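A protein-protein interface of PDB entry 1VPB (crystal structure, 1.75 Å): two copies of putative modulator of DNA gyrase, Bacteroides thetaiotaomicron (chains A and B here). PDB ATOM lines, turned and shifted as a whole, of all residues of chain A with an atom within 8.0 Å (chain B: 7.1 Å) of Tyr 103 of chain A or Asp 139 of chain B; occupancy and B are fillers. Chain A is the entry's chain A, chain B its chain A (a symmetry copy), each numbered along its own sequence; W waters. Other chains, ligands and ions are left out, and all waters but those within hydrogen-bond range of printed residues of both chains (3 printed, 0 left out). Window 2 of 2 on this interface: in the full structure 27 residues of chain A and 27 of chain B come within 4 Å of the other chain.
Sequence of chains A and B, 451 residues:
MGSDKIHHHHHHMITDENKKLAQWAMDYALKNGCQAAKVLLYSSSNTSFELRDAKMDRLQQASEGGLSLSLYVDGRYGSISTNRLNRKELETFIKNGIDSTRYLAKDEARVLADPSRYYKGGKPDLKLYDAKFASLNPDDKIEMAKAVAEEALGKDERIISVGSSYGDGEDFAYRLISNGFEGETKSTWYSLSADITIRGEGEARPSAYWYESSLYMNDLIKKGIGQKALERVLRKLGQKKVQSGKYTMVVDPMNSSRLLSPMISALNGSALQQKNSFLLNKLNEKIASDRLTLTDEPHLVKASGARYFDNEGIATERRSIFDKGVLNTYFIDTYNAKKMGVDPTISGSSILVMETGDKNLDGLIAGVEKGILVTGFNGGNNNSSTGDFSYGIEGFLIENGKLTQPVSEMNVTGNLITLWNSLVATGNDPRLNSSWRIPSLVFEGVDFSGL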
ATOM      1  N   VAL A  73      -0.043 -16.011  23.724  1.00  0.00           N
ATOM      2  CA  VAL A  73       0.967 -16.735  22.944  1.00  0.00           C
ATOM      3  C   VAL A  73       2.179 -16.941  23.823  1.00  0.00           C
ATOM      4  O   VAL A  73       3.018 -16.038  24.120  1.00  0.00           O
ATOM      5  CB  VAL A  73       1.422 -15.957  21.672  1.00  0.00           C
ATOM      6  CG1 VAL A  73       2.458 -16.796  20.889  1.00  0.00           C
ATOM      7  CG2 VAL A  73       0.247 -15.538  20.811  1.00  0.00           C
ATOM      8  N   ASP A  74       2.324 -18.166  24.297  1.00  0.00           N
ATOM      9  CA  ASP A  74       3.517 -18.437  25.080  1.00  0.00           C
ATOM     10  C   ASP A  74       3.763 -17.561  26.259  1.00  0.00           C
ATOM     11  O   ASP A  74       4.893 -17.204  26.591  1.00  0.00           O
ATOM     12  CB  ASP A  74       4.759 -18.557  24.157  1.00  0.00           C
ATOM     13  CG  ASP A  74       4.629 -19.629  23.102  1.00  0.00           C
ATOM     14  OD1 ASP A  74       3.602 -20.413  22.999  1.00  0.00           O
ATOM     15  OD2 ASP A  74       5.524 -19.705  22.211  1.00  0.00           O
ATOM     16  N   ARG A  76       2.840 -14.497  26.535  1.00  0.00           N
ATOM     17  CA  ARG A  76       2.755 -13.126  26.067  1.00  0.00           C
ATOM     18  C   ARG A  76       1.290 -12.799  25.737  1.00  0.00           C
ATOM     19  O   ARG A  76       0.470 -13.673  25.440  1.00  0.00           O
ATOM     20  CB  ARG A  76       3.631 -12.901  24.852  1.00  0.00           C
ATOM     21  CG  ARG A  76       5.089 -12.905  25.158  1.00  0.00           C
ATOM     22  CD  ARG A  76       5.699 -14.299  25.378  1.00  0.00           C
ATOM     23  NE  ARG A  76       7.125 -14.258  25.310  1.00  0.00           N
ATOM     24  CZ  ARG A  76       7.959 -15.332  25.333  1.00  0.00           C
ATOM     25  NH1 ARG A  76       7.439 -16.539  25.428  1.00  0.00           N
ATOM     26  NH2 ARG A  76       9.262 -15.178  25.140  1.00  0.00           N
ATOM     27  N   ASN A  96       0.962 -13.177  11.694  1.00  0.00           N
ATOM     28  CA  ASN A  96       1.945 -12.146  11.990  1.00  0.00           C
ATOM     29  C   ASN A  96       1.737 -11.576  13.375  1.00  0.00           C
ATOM     30  O   ASN A  96       2.708 -11.353  14.056  1.00  0.00           O
ATOM     31  CB  ASN A  96       1.924 -11.049  10.946  1.00  0.00           C
ATOM     32  CG  ASN A  96       2.533 -11.516   9.631  1.00  0.00           C
ATOM     33  OD1 ASN A  96       3.186 -12.591   9.562  1.00  0.00           O
ATOM     34  ND2 ASN A  96       2.356 -10.716   8.581  1.00  0.00           N
ATOM     35  N   GLY A  97       0.478 -11.391  13.804  1.00  0.00           N
ATOM     36  CA  GLY A  97       0.179 -10.942  15.140  1.00  0.00           C
ATOM     37  C   GLY A  97       0.659 -11.899  16.233  1.00  0.00           C
ATOM     38  O   GLY A  97       1.253 -11.476  17.234  1.00  0.00           O
ATOM     39  N   ILE A  98       0.459 -13.188  15.978  1.00  0.00           N
ATOM     40  CA  ILE A  98       0.883 -14.228  16.918  1.00  0.00           C
ATOM     41  C   ILE A  98       2.408 -14.211  17.073  1.00  0.00           C
ATOM     42  O   ILE A  98       2.945 -14.176  18.175  1.00  0.00           O
ATOM     43  CB  ILE A  98       0.370 -15.619  16.449  1.00  0.00           C
ATOM     44  CG1 ILE A  98      -1.139 -15.707  16.598  1.00  0.00           C
ATOM     45  CG2 ILE A  98       1.032 -16.714  17.219  1.00  0.00           C
ATOM     46  CD1 ILE A  98      -1.794 -16.936  15.980  1.00  0.00           C
ATOM     47  N   ASP A  99       3.094 -14.189  15.934  1.00  0.00           N
ATOM     48  CA  ASP A  99       4.542 -14.267  15.934  1.00  0.00           C
ATOM     49  C   ASP A  99       5.171 -12.999  16.526  1.00  0.00           C
ATOM     50  O   ASP A  99       6.117 -13.074  17.268  1.00  0.00           O
ATOM     51  CB  ASP A  99       5.018 -14.553  14.561  1.00  0.00           C
ATOM     52  CG  ASP A  99       4.733 -15.989  14.114  1.00  0.00           C
ATOM     53  OD1 ASP A  99       4.536 -16.933  14.937  1.00  0.00           O
ATOM     54  OD2 ASP A  99       4.718 -16.241  12.898  1.00  0.00           O
ATOM     55  N   SER A 100       4.532 -11.852  16.287  1.00  0.00           N
ATOM     56  CA  SER A 100       4.966 -10.596  16.863  1.00  0.00           C
ATOM     57  C   SER A 100       4.756 -10.555  18.384  1.00  0.00           C
ATOM     58  O   SER A 100       5.622 -10.076  19.129  1.00  0.00           O
ATOM     59  CB  SER A 100       4.195  -9.473  16.208  1.00  0.00           C
ATOM     60  OG  SER A 100       4.587  -9.360  14.865  1.00  0.00           O
ATOM     61  N   THR A 101       3.644 -11.073  18.819  1.00  0.00           N
ATOM     62  CA  THR A 101       3.281 -11.108  20.244  1.00  0.00           C
ATOM     63  C   THR A 101       4.301 -11.919  21.004  1.00  0.00           C
ATOM     64  O   THR A 101       4.705 -11.566  22.106  1.00  0.00           O
ATOM     65  CB  THR A 101       1.887 -11.706  20.440  1.00  0.00           C
ATOM     66  OG1 THR A 101       0.877 -10.829  19.914  1.00  0.00           O
ATOM     67  CG2 THR A 101       1.505 -12.001  21.872  1.00  0.00           C
ATOM     68  N   ARG A 102       4.745 -13.013  20.391  1.00  0.00           N
ATOM     69  CA  ARG A 102       5.718 -13.873  21.083  1.00  0.00           C
ATOM     70  C   ARG A 102       7.041 -13.193  21.425  1.00  0.00           C
ATOM     71  O   ARG A 102       7.832 -13.649  22.267  1.00  0.00           O
ATOM     72  CB  ARG A 102       5.955 -15.124  20.239  1.00  0.00           C
ATOM     73  CG  ARG A 102       6.630 -16.249  20.997  1.00  0.00           C
ATOM     74  CD  ARG A 102       6.916 -17.525  20.197  1.00  0.00           C
ATOM     75  NE  ARG A 102       5.702 -18.254  19.811  1.00  0.00           N
ATOM     76  CZ  ARG A 102       5.144 -18.241  18.605  1.00  0.00           C
ATOM     77  NH1 ARG A 102       5.605 -17.507  17.614  1.00  0.00           N
ATOM     78  NH2 ARG A 102       4.077 -18.940  18.408  1.00  0.00           N
ATOM     79  N   TYR A 103       7.384 -12.132  20.681  1.00  0.00           N
ATOM     80  CA  TYR A 103       8.590 -11.383  20.967  1.00  0.00           C
ATOM     81  C   TYR A 103       8.540 -10.483  22.210  1.00  0.00           C
ATOM     82  O   TYR A 103       9.622 -10.016  22.729  1.00  0.00           O
ATOM     83  CB  TYR A 103       9.009 -10.544  19.774  1.00  0.00           C
ATOM     84  CG  TYR A 103       9.272 -11.361  18.518  1.00  0.00           C
ATOM     85  CD1 TYR A 103      10.253 -12.350  18.484  1.00  0.00           C
ATOM     86  CD2 TYR A 103       8.603 -11.072  17.389  1.00  0.00           C
ATOM     87  CE1 TYR A 103      10.488 -13.076  17.288  1.00  0.00           C
ATOM     88  CE2 TYR A 103       8.834 -11.770  16.209  1.00  0.00           C
ATOM     89  CZ  TYR A 103       9.757 -12.764  16.176  1.00  0.00           C
ATOM     90  OH  TYR A 103       9.955 -13.404  14.933  1.00  0.00           O
ATOM     91  N   LEU A 104       7.346 -10.257  22.703  1.00  0.00           N
ATOM     92  CA  LEU A 104       7.151  -9.492  23.950  1.00  0.00           C
ATOM     93  C   LEU A 104       7.746 -10.257  25.139  1.00  0.00           C
ATOM     94  O   LEU A 104       7.974 -11.472  25.058  1.00  0.00           O
ATOM     95  CB  LEU A 104       5.675  -9.279  24.214  1.00  0.00           C
ATOM     96  CG  LEU A 104       4.917  -8.451  23.201  1.00  0.00           C
ATOM     97  CD1 LEU A 104       3.455  -8.417  23.514  1.00  0.00           C
ATOM     98  CD2 LEU A 104       5.478  -7.084  23.001  1.00  0.00           C
ATOM     99  N   ALA A 105       7.942  -9.573  26.247  1.00  0.00           N
ATOM    100  CA  ALA A 105       8.180 -10.271  27.510  1.00  0.00           C
ATOM    101  C   ALA A 105       6.932 -10.892  27.966  1.00  0.00           C
ATOM    102  O   ALA A 105       5.854 -10.334  27.830  1.00  0.00           O
ATOM    103  CB  ALA A 105       8.699  -9.307  28.572  1.00  0.00           C
ATOM    104  N   LYS A 106       7.027 -12.095  28.517  1.00  0.00           N
ATOM    105  CA  LYS A 106       5.821 -12.723  28.993  1.00  0.00           C
ATOM    106  C   LYS A 106       5.206 -11.973  30.182  1.00  0.00           C
ATOM    107  O   LYS A 106       5.892 -11.295  30.950  1.00  0.00           O
ATOM    108  CB  LYS A 106       6.069 -14.208  29.319  1.00  0.00           C
ATOM    109  CG  LYS A 106       6.891 -14.457  30.461  1.00  0.00           C
ATOM    110  CD  LYS A 106       7.223 -15.994  30.582  1.00  0.00           C
ATOM    111  CE  LYS A 106       7.827 -16.169  31.984  1.00  0.00           C
ATOM    112  NZ  LYS A 106       8.253 -17.564  32.248  1.00  0.00           N
ATOM    113  N   PHE B  49       4.755  -0.919  19.505  1.00  0.00           N
ATOM    114  CA  PHE B  49       5.254  -1.544  20.718  1.00  0.00           C
ATOM    115  C   PHE B  49       5.444  -0.447  21.769  1.00  0.00           C
ATOM    116  O   PHE B  49       6.127   0.543  21.507  1.00  0.00           O
ATOM    117  CB  PHE B  49       6.626  -2.237  20.570  1.00  0.00           C
ATOM    118  CG  PHE B  49       6.611  -3.492  19.726  1.00  0.00           C
ATOM    119  CD1 PHE B  49       6.221  -4.718  20.285  1.00  0.00           C
ATOM    120  CD2 PHE B  49       7.048  -3.477  18.393  1.00  0.00           C
ATOM    121  CE1 PHE B  49       6.216  -5.911  19.484  1.00  0.00           C
ATOM    122  CE2 PHE B  49       7.013  -4.628  17.600  1.00  0.00           C
ATOM    123  CZ  PHE B  49       6.590  -5.849  18.149  1.00  0.00           C
ATOM    124  N   ASP B  57       5.130  -4.836  28.638  1.00  0.00           N
ATOM    125  CA  ASP B  57       5.243  -4.827  27.170  1.00  0.00           C
ATOM    126  C   ASP B  57       3.875  -4.830  26.562  1.00  0.00           C
ATOM    127  O   ASP B  57       3.005  -5.611  26.941  1.00  0.00           O
ATOM    128  CB  ASP B  57       5.918  -6.080  26.654  1.00  0.00           C
ATOM    129  CG  ASP B  57       7.392  -6.052  26.810  1.00  0.00           C
ATOM    130  OD1 ASP B  57       7.920  -5.188  27.545  1.00  0.00           O
ATOM    131  OD2 ASP B  57       8.123  -6.861  26.231  1.00  0.00           O
ATOM    132  N   LEU B  59       1.819  -4.687  22.658  1.00  0.00           N
ATOM    133  CA  LEU B  59       1.805  -4.717  21.211  1.00  0.00           C
ATOM    134  C   LEU B  59       0.389  -4.446  20.718  1.00  0.00           C
ATOM    135  O   LEU B  59      -0.567  -5.122  21.153  1.00  0.00           O
ATOM    136  CB  LEU B  59       2.120  -6.110  20.711  1.00  0.00           C
ATOM    137  CG  LEU B  59       2.019  -6.291  19.211  1.00  0.00           C
ATOM    138  CD1 LEU B  59       3.007  -5.402  18.402  1.00  0.00           C
ATOM    139  CD2 LEU B  59       2.259  -7.691  18.925  1.00  0.00           C
ATOM    140  N   LEU B 136      10.376  -6.325   7.256  1.00  0.00           N
ATOM    141  CA  LEU B 136      11.059  -6.030   8.531  1.00  0.00           C
ATOM    142  C   LEU B 136      10.600  -7.014   9.569  1.00  0.00           C
ATOM    143  O   LEU B 136       9.471  -7.519   9.468  1.00  0.00           O
ATOM    144  CB  LEU B 136      10.732  -4.618   9.038  1.00  0.00           C
ATOM    145  CG  LEU B 136      11.236  -3.541   8.088  1.00  0.00           C
ATOM    146  CD1 LEU B 136      10.769  -2.187   8.592  1.00  0.00           C
ATOM    147  CD2 LEU B 136      12.737  -3.628   8.022  1.00  0.00           C
ATOM    148  N   ASN B 137      11.483  -7.310  10.506  1.00  0.00           N
ATOM    149  CA  ASN B 137      11.259  -8.345  11.510  1.00  0.00           C
ATOM    150  C   ASN B 137      10.782  -7.646  12.798  1.00  0.00           C
ATOM    151  O   ASN B 137      11.459  -6.754  13.321  1.00  0.00           O
ATOM    152  CB  ASN B 137      12.573  -9.081  11.798  1.00  0.00           C
ATOM    153  CG  ASN B 137      12.448 -10.131  12.915  1.00  0.00           C
ATOM    154  OD1 ASN B 137      11.382 -10.305  13.524  1.00  0.00           O
ATOM    155  ND2 ASN B 137      13.555 -10.844  13.185  1.00  0.00           N
ATOM    156  N   PRO B 138       9.605  -8.012  13.296  1.00  0.00           N
ATOM    157  CA  PRO B 138       9.055  -7.341  14.473  1.00  0.00           C
ATOM    158  C   PRO B 138       9.993  -7.427  15.634  1.00  0.00           C
ATOM    159  O   PRO B 138      10.042  -6.541  16.494  1.00  0.00           O
ATOM    160  CB  PRO B 138       7.756  -8.144  14.736  1.00  0.00           C
ATOM    161  CG  PRO B 138       7.347  -8.548  13.357  1.00  0.00           C
ATOM    162  CD  PRO B 138       8.676  -9.016  12.767  1.00  0.00           C
ATOM    163  N   ASP B 139      10.773  -8.475  15.711  1.00  0.00           N
ATOM    164  CA  ASP B 139      11.712  -8.560  16.801  1.00  0.00           C
ATOM    165  C   ASP B 139      12.798  -7.474  16.836  1.00  0.00           C
ATOM    166  O   ASP B 139      13.223  -7.011  17.904  1.00  0.00           O
ATOM    167  CB  ASP B 139      12.350  -9.945  16.765  1.00  0.00           C
ATOM    168  CG  ASP B 139      12.971 -10.344  18.079  1.00  0.00           C
ATOM    169  OD1 ASP B 139      12.549  -9.856  19.183  1.00  0.00           O
ATOM    170  OD2 ASP B 139      13.898 -11.174  18.086  1.00  0.00           O
ATOM    171  N   ASP B 140      13.263  -7.039  15.662  1.00  0.00           N
ATOM    172  CA  ASP B 140      14.189  -5.899  15.595  1.00  0.00           C
ATOM    173  C   ASP B 140      13.532  -4.586  16.063  1.00  0.00           C
ATOM    174  O   ASP B 140      14.160  -3.745  16.693  1.00  0.00           O
ATOM    175  CB  ASP B 140      14.666  -5.727  14.154  1.00  0.00           C
ATOM    176  CG  ASP B 140      15.484  -6.908  13.667  1.00  0.00           C
ATOM    177  OD1 ASP B 140      16.127  -7.571  14.485  1.00  0.00           O
ATOM    178  OD2 ASP B 140      15.546  -7.205  12.469  1.00  0.00           O
ATOM    179  N   LYS B 141      12.249  -4.449  15.745  1.00  0.00           N
ATOM    180  CA  LYS B 141      11.459  -3.265  16.116  1.00  0.00           C
ATOM    181  C   LYS B 141      11.380  -3.172  17.642  1.00  0.00           C
ATOM    182  O   LYS B 141      11.735  -2.157  18.242  1.00  0.00           O
ATOM    183  CB  LYS B 141      10.060  -3.323  15.464  1.00  0.00           C
ATOM    184  CG  LYS B 141      10.023  -3.402  13.939  1.00  0.00           C
ATOM    185  CD  LYS B 141       8.626  -3.506  13.456  1.00  0.00           C
ATOM    186  CE  LYS B 141       8.548  -3.760  11.974  1.00  0.00           C
ATOM    187  NZ  LYS B 141       7.197  -3.765  11.391  1.00  0.00           N
ATOM    188  N   ILE B 142      10.938  -4.237  18.297  1.00  0.00           N
ATOM    189  CA  ILE B 142      10.845  -4.166  19.743  1.00  0.00           C
ATOM    190  C   ILE B 142      12.225  -4.046  20.415  1.00  0.00           C
ATOM    191  O   ILE B 142      12.363  -3.375  21.439  1.00  0.00           O
ATOM    192  CB  ILE B 142      10.030  -5.335  20.315  1.00  0.00           C
ATOM    193  CG1 ILE B 142       9.662  -5.018  21.758  1.00  0.00           C
ATOM    194  CG2 ILE B 142      10.808  -6.636  20.221  1.00  0.00           C
ATOM    195  CD1 ILE B 142       9.029  -6.133  22.482  1.00  0.00           C
ATOM    196  N   GLU B 143      13.261  -4.650  19.838  1.00  0.00           N
ATOM    197  CA  GLU B 143      14.620  -4.433  20.344  1.00  0.00           C
ATOM    198  C   GLU B 143      15.063  -2.963  20.334  1.00  0.00           C
ATOM    199  O   GLU B 143      15.776  -2.489  21.264  1.00  0.00           O
ATOM    200  CB  GLU B 143      15.660  -5.253  19.567  1.00  0.00           C
ATOM    201  CG  GLU B 143      15.651  -6.746  19.859  1.00  0.00           C
ATOM    202  CD  GLU B 143      15.841  -7.091  21.332  1.00  0.00           C
ATOM    203  OE1 GLU B 143      16.725  -6.484  21.982  1.00  0.00           O
ATOM    204  OE2 GLU B 143      15.077  -7.956  21.837  1.00  0.00           O
ATOM    205  N   MET B 144      14.728  -2.243  19.265  1.00  0.00           N
ATOM    206  CA  MET B 144      15.020  -0.810  19.227  1.00  0.00           C
ATOM    207  C   MET B 144      14.388  -0.075  20.391  1.00  0.00           C
ATOM    208  O   MET B 144      15.016   0.802  20.948  1.00  0.00           O
ATOM    209  CB  MET B 144      14.547  -0.165  17.931  1.00  0.00           C
ATOM    210  CG  MET B 144      15.271  -0.664  16.697  1.00  0.00           C
ATOM    211  SD  MET B 144      14.583  -0.027  15.158  1.00  0.00           S
ATOM    212  CE  MET B 144      15.212  -1.211  14.048  1.00  0.00           C
ATOM    213  N   LYS B 146      13.523  -1.363  23.289  1.00  0.00           N
ATOM    214  CA  LYS B 146      14.287  -1.756  24.450  1.00  0.00           C
ATOM    215  C   LYS B 146      15.600  -0.999  24.582  1.00  0.00           C
ATOM    216  O   LYS B 146      15.957  -0.557  25.669  1.00  0.00           O
ATOM    217  CB  LYS B 146      14.615  -3.232  24.398  1.00  0.00           C
ATOM    218  CG  LYS B 146      13.474  -4.136  24.476  1.00  0.00           C
ATOM    219  CD  LYS B 146      14.025  -5.545  24.760  1.00  0.00           C
ATOM    220  CE  LYS B 146      13.218  -6.588  24.053  1.00  0.00           C
ATOM    221  NZ  LYS B 146      13.608  -7.945  24.560  1.00  0.00           N
HETATM  222  O   HOH W   1      11.033  -8.532  24.577  1.00  0.00           O
HETATM  223  O   HOH W   2       5.053  -8.027  29.266  1.00  0.00           O
HETATM  224  O   HOH W   3      12.071 -10.688  21.785  1.00  0.00           O
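N of Ala 105 of chain A is in hydrogen-bond range of OD2 of Asp 57 of chain B, at 2.7 Å.
The backbone carbonyl oxygen (O) of Leu 104 of chain A is in hydrogen-bond range of the guanidinium group (NE) of Arg 76 of chain A (2.9 Å).
The backbone carbonyl oxygen (O) of Asn 96 of chain A sits at hydrogen-bond distance from the side-chain hydroxyl (OG) of Ser 100 of chain A (2.9 Å).
The backbone carbonyl oxygen of Gly 97 of chain A sits at hydrogen-bond distance from the side-chain hydroxyl of Thr 101 of chain A (2.8 Å).
OD1 of Asn 137 of chain B lies within hydrogen-bond range of N of Asp 139 of chain B, at 2.9 Å.
Among the printed residues, pairs that only touch across the chains: Ser 100 of chain A with Pro 138 of chain B (3.2 Å), Tyr 103 of chain A with Asp 139 of chain B (3.4 Å), Thr 101 of chain A with Leu 59 of chain B (3.6 Å), Leu 104 of chain A with Asp 57 of chain B (3.6 Å), Leu 104 of chain A with Phe 49 of chain B (3.7 Å), Tyr 103 of chain A with Asn 137 of chain B (3.7 Å), Leu 104 of chain A with Ile 142 of chain B (3.7 Å), Ser 100 of chain A with Leu 59 of chain B (3.8 Å), Leu 104 of chain A with Leu 59 of chain B (3.9 Å) and Tyr 103 of chain A with Ile 142 of chain B (3.9 Å).
Arg 76 of chain A touches none of the printed residues of chain B.
Gly 97 of chain A touches none of the printed residues of chain B.
Of the printed residues of chain B, Tyr 103 of chain A touches Asn 137, Asp 139 and Ile 142.
Printed residues of chain B within 4 Å of Ala 105 of chain A: Asp 57.
Printed residues of chain A within 4 Å of Asp 57 of chain B: Leu 104 (3.6 Å) and Ala 105 (2.7 Å).
Of chain A, only Tyr 103 comes within 4 Å of Asp 139 of chain B.
Printed residues of chain A within 4 Å of Ile 142 of chain B: Tyr 103 and Leu 104.
The nearest printed residue of chain B that does not touch Ser 100 of chain A is Phe 49 of chain B (4.2 Å).
Hydrophobic or aromatic side chains of chain A that line the printed part of chain B: Tyr 103, Leu 104 and Ala 105.
Of the 13 printed residues of chain B, 7 touch a printed residue of chain A.
Printed residues of chain B that touch a printed residue of chain A: Phe 49, Asp 57, Leu 59, Asn 137, Pro 138, Asp 139 and Ile 142.
Hydrophobic or aromatic side chains of chain B within 4 Å of the printed part of chain A: Phe 49, Leu 59, Pro 138 and Ile 142.
Among the printed residues, 11 pairs touch across the chains.
Among the printed residues, no Asp or Glu carboxylate lies within 4 Å of a Lys or Arg side-chain nitrogen of the other chain.
No position is printed for both chains.
Water W1 lies within hydrogen-bond range of the side-chain amino group (NZ) of Lys 146 of chain B (2.6 Å) and the backbone carbonyl oxygen (O) of Tyr 103 of chain A (2.8 Å).
Water W3 lies within hydrogen-bond range of O of Tyr 103 of chain A (2.7 Å) and OD1 of Asp 139 of chain B (2.8 Å).
Water W2 lies within hydrogen-bond range of O of Ala 105 of chain A (2.8 Å) and N of Asp 57 of chain B (3.3 Å).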
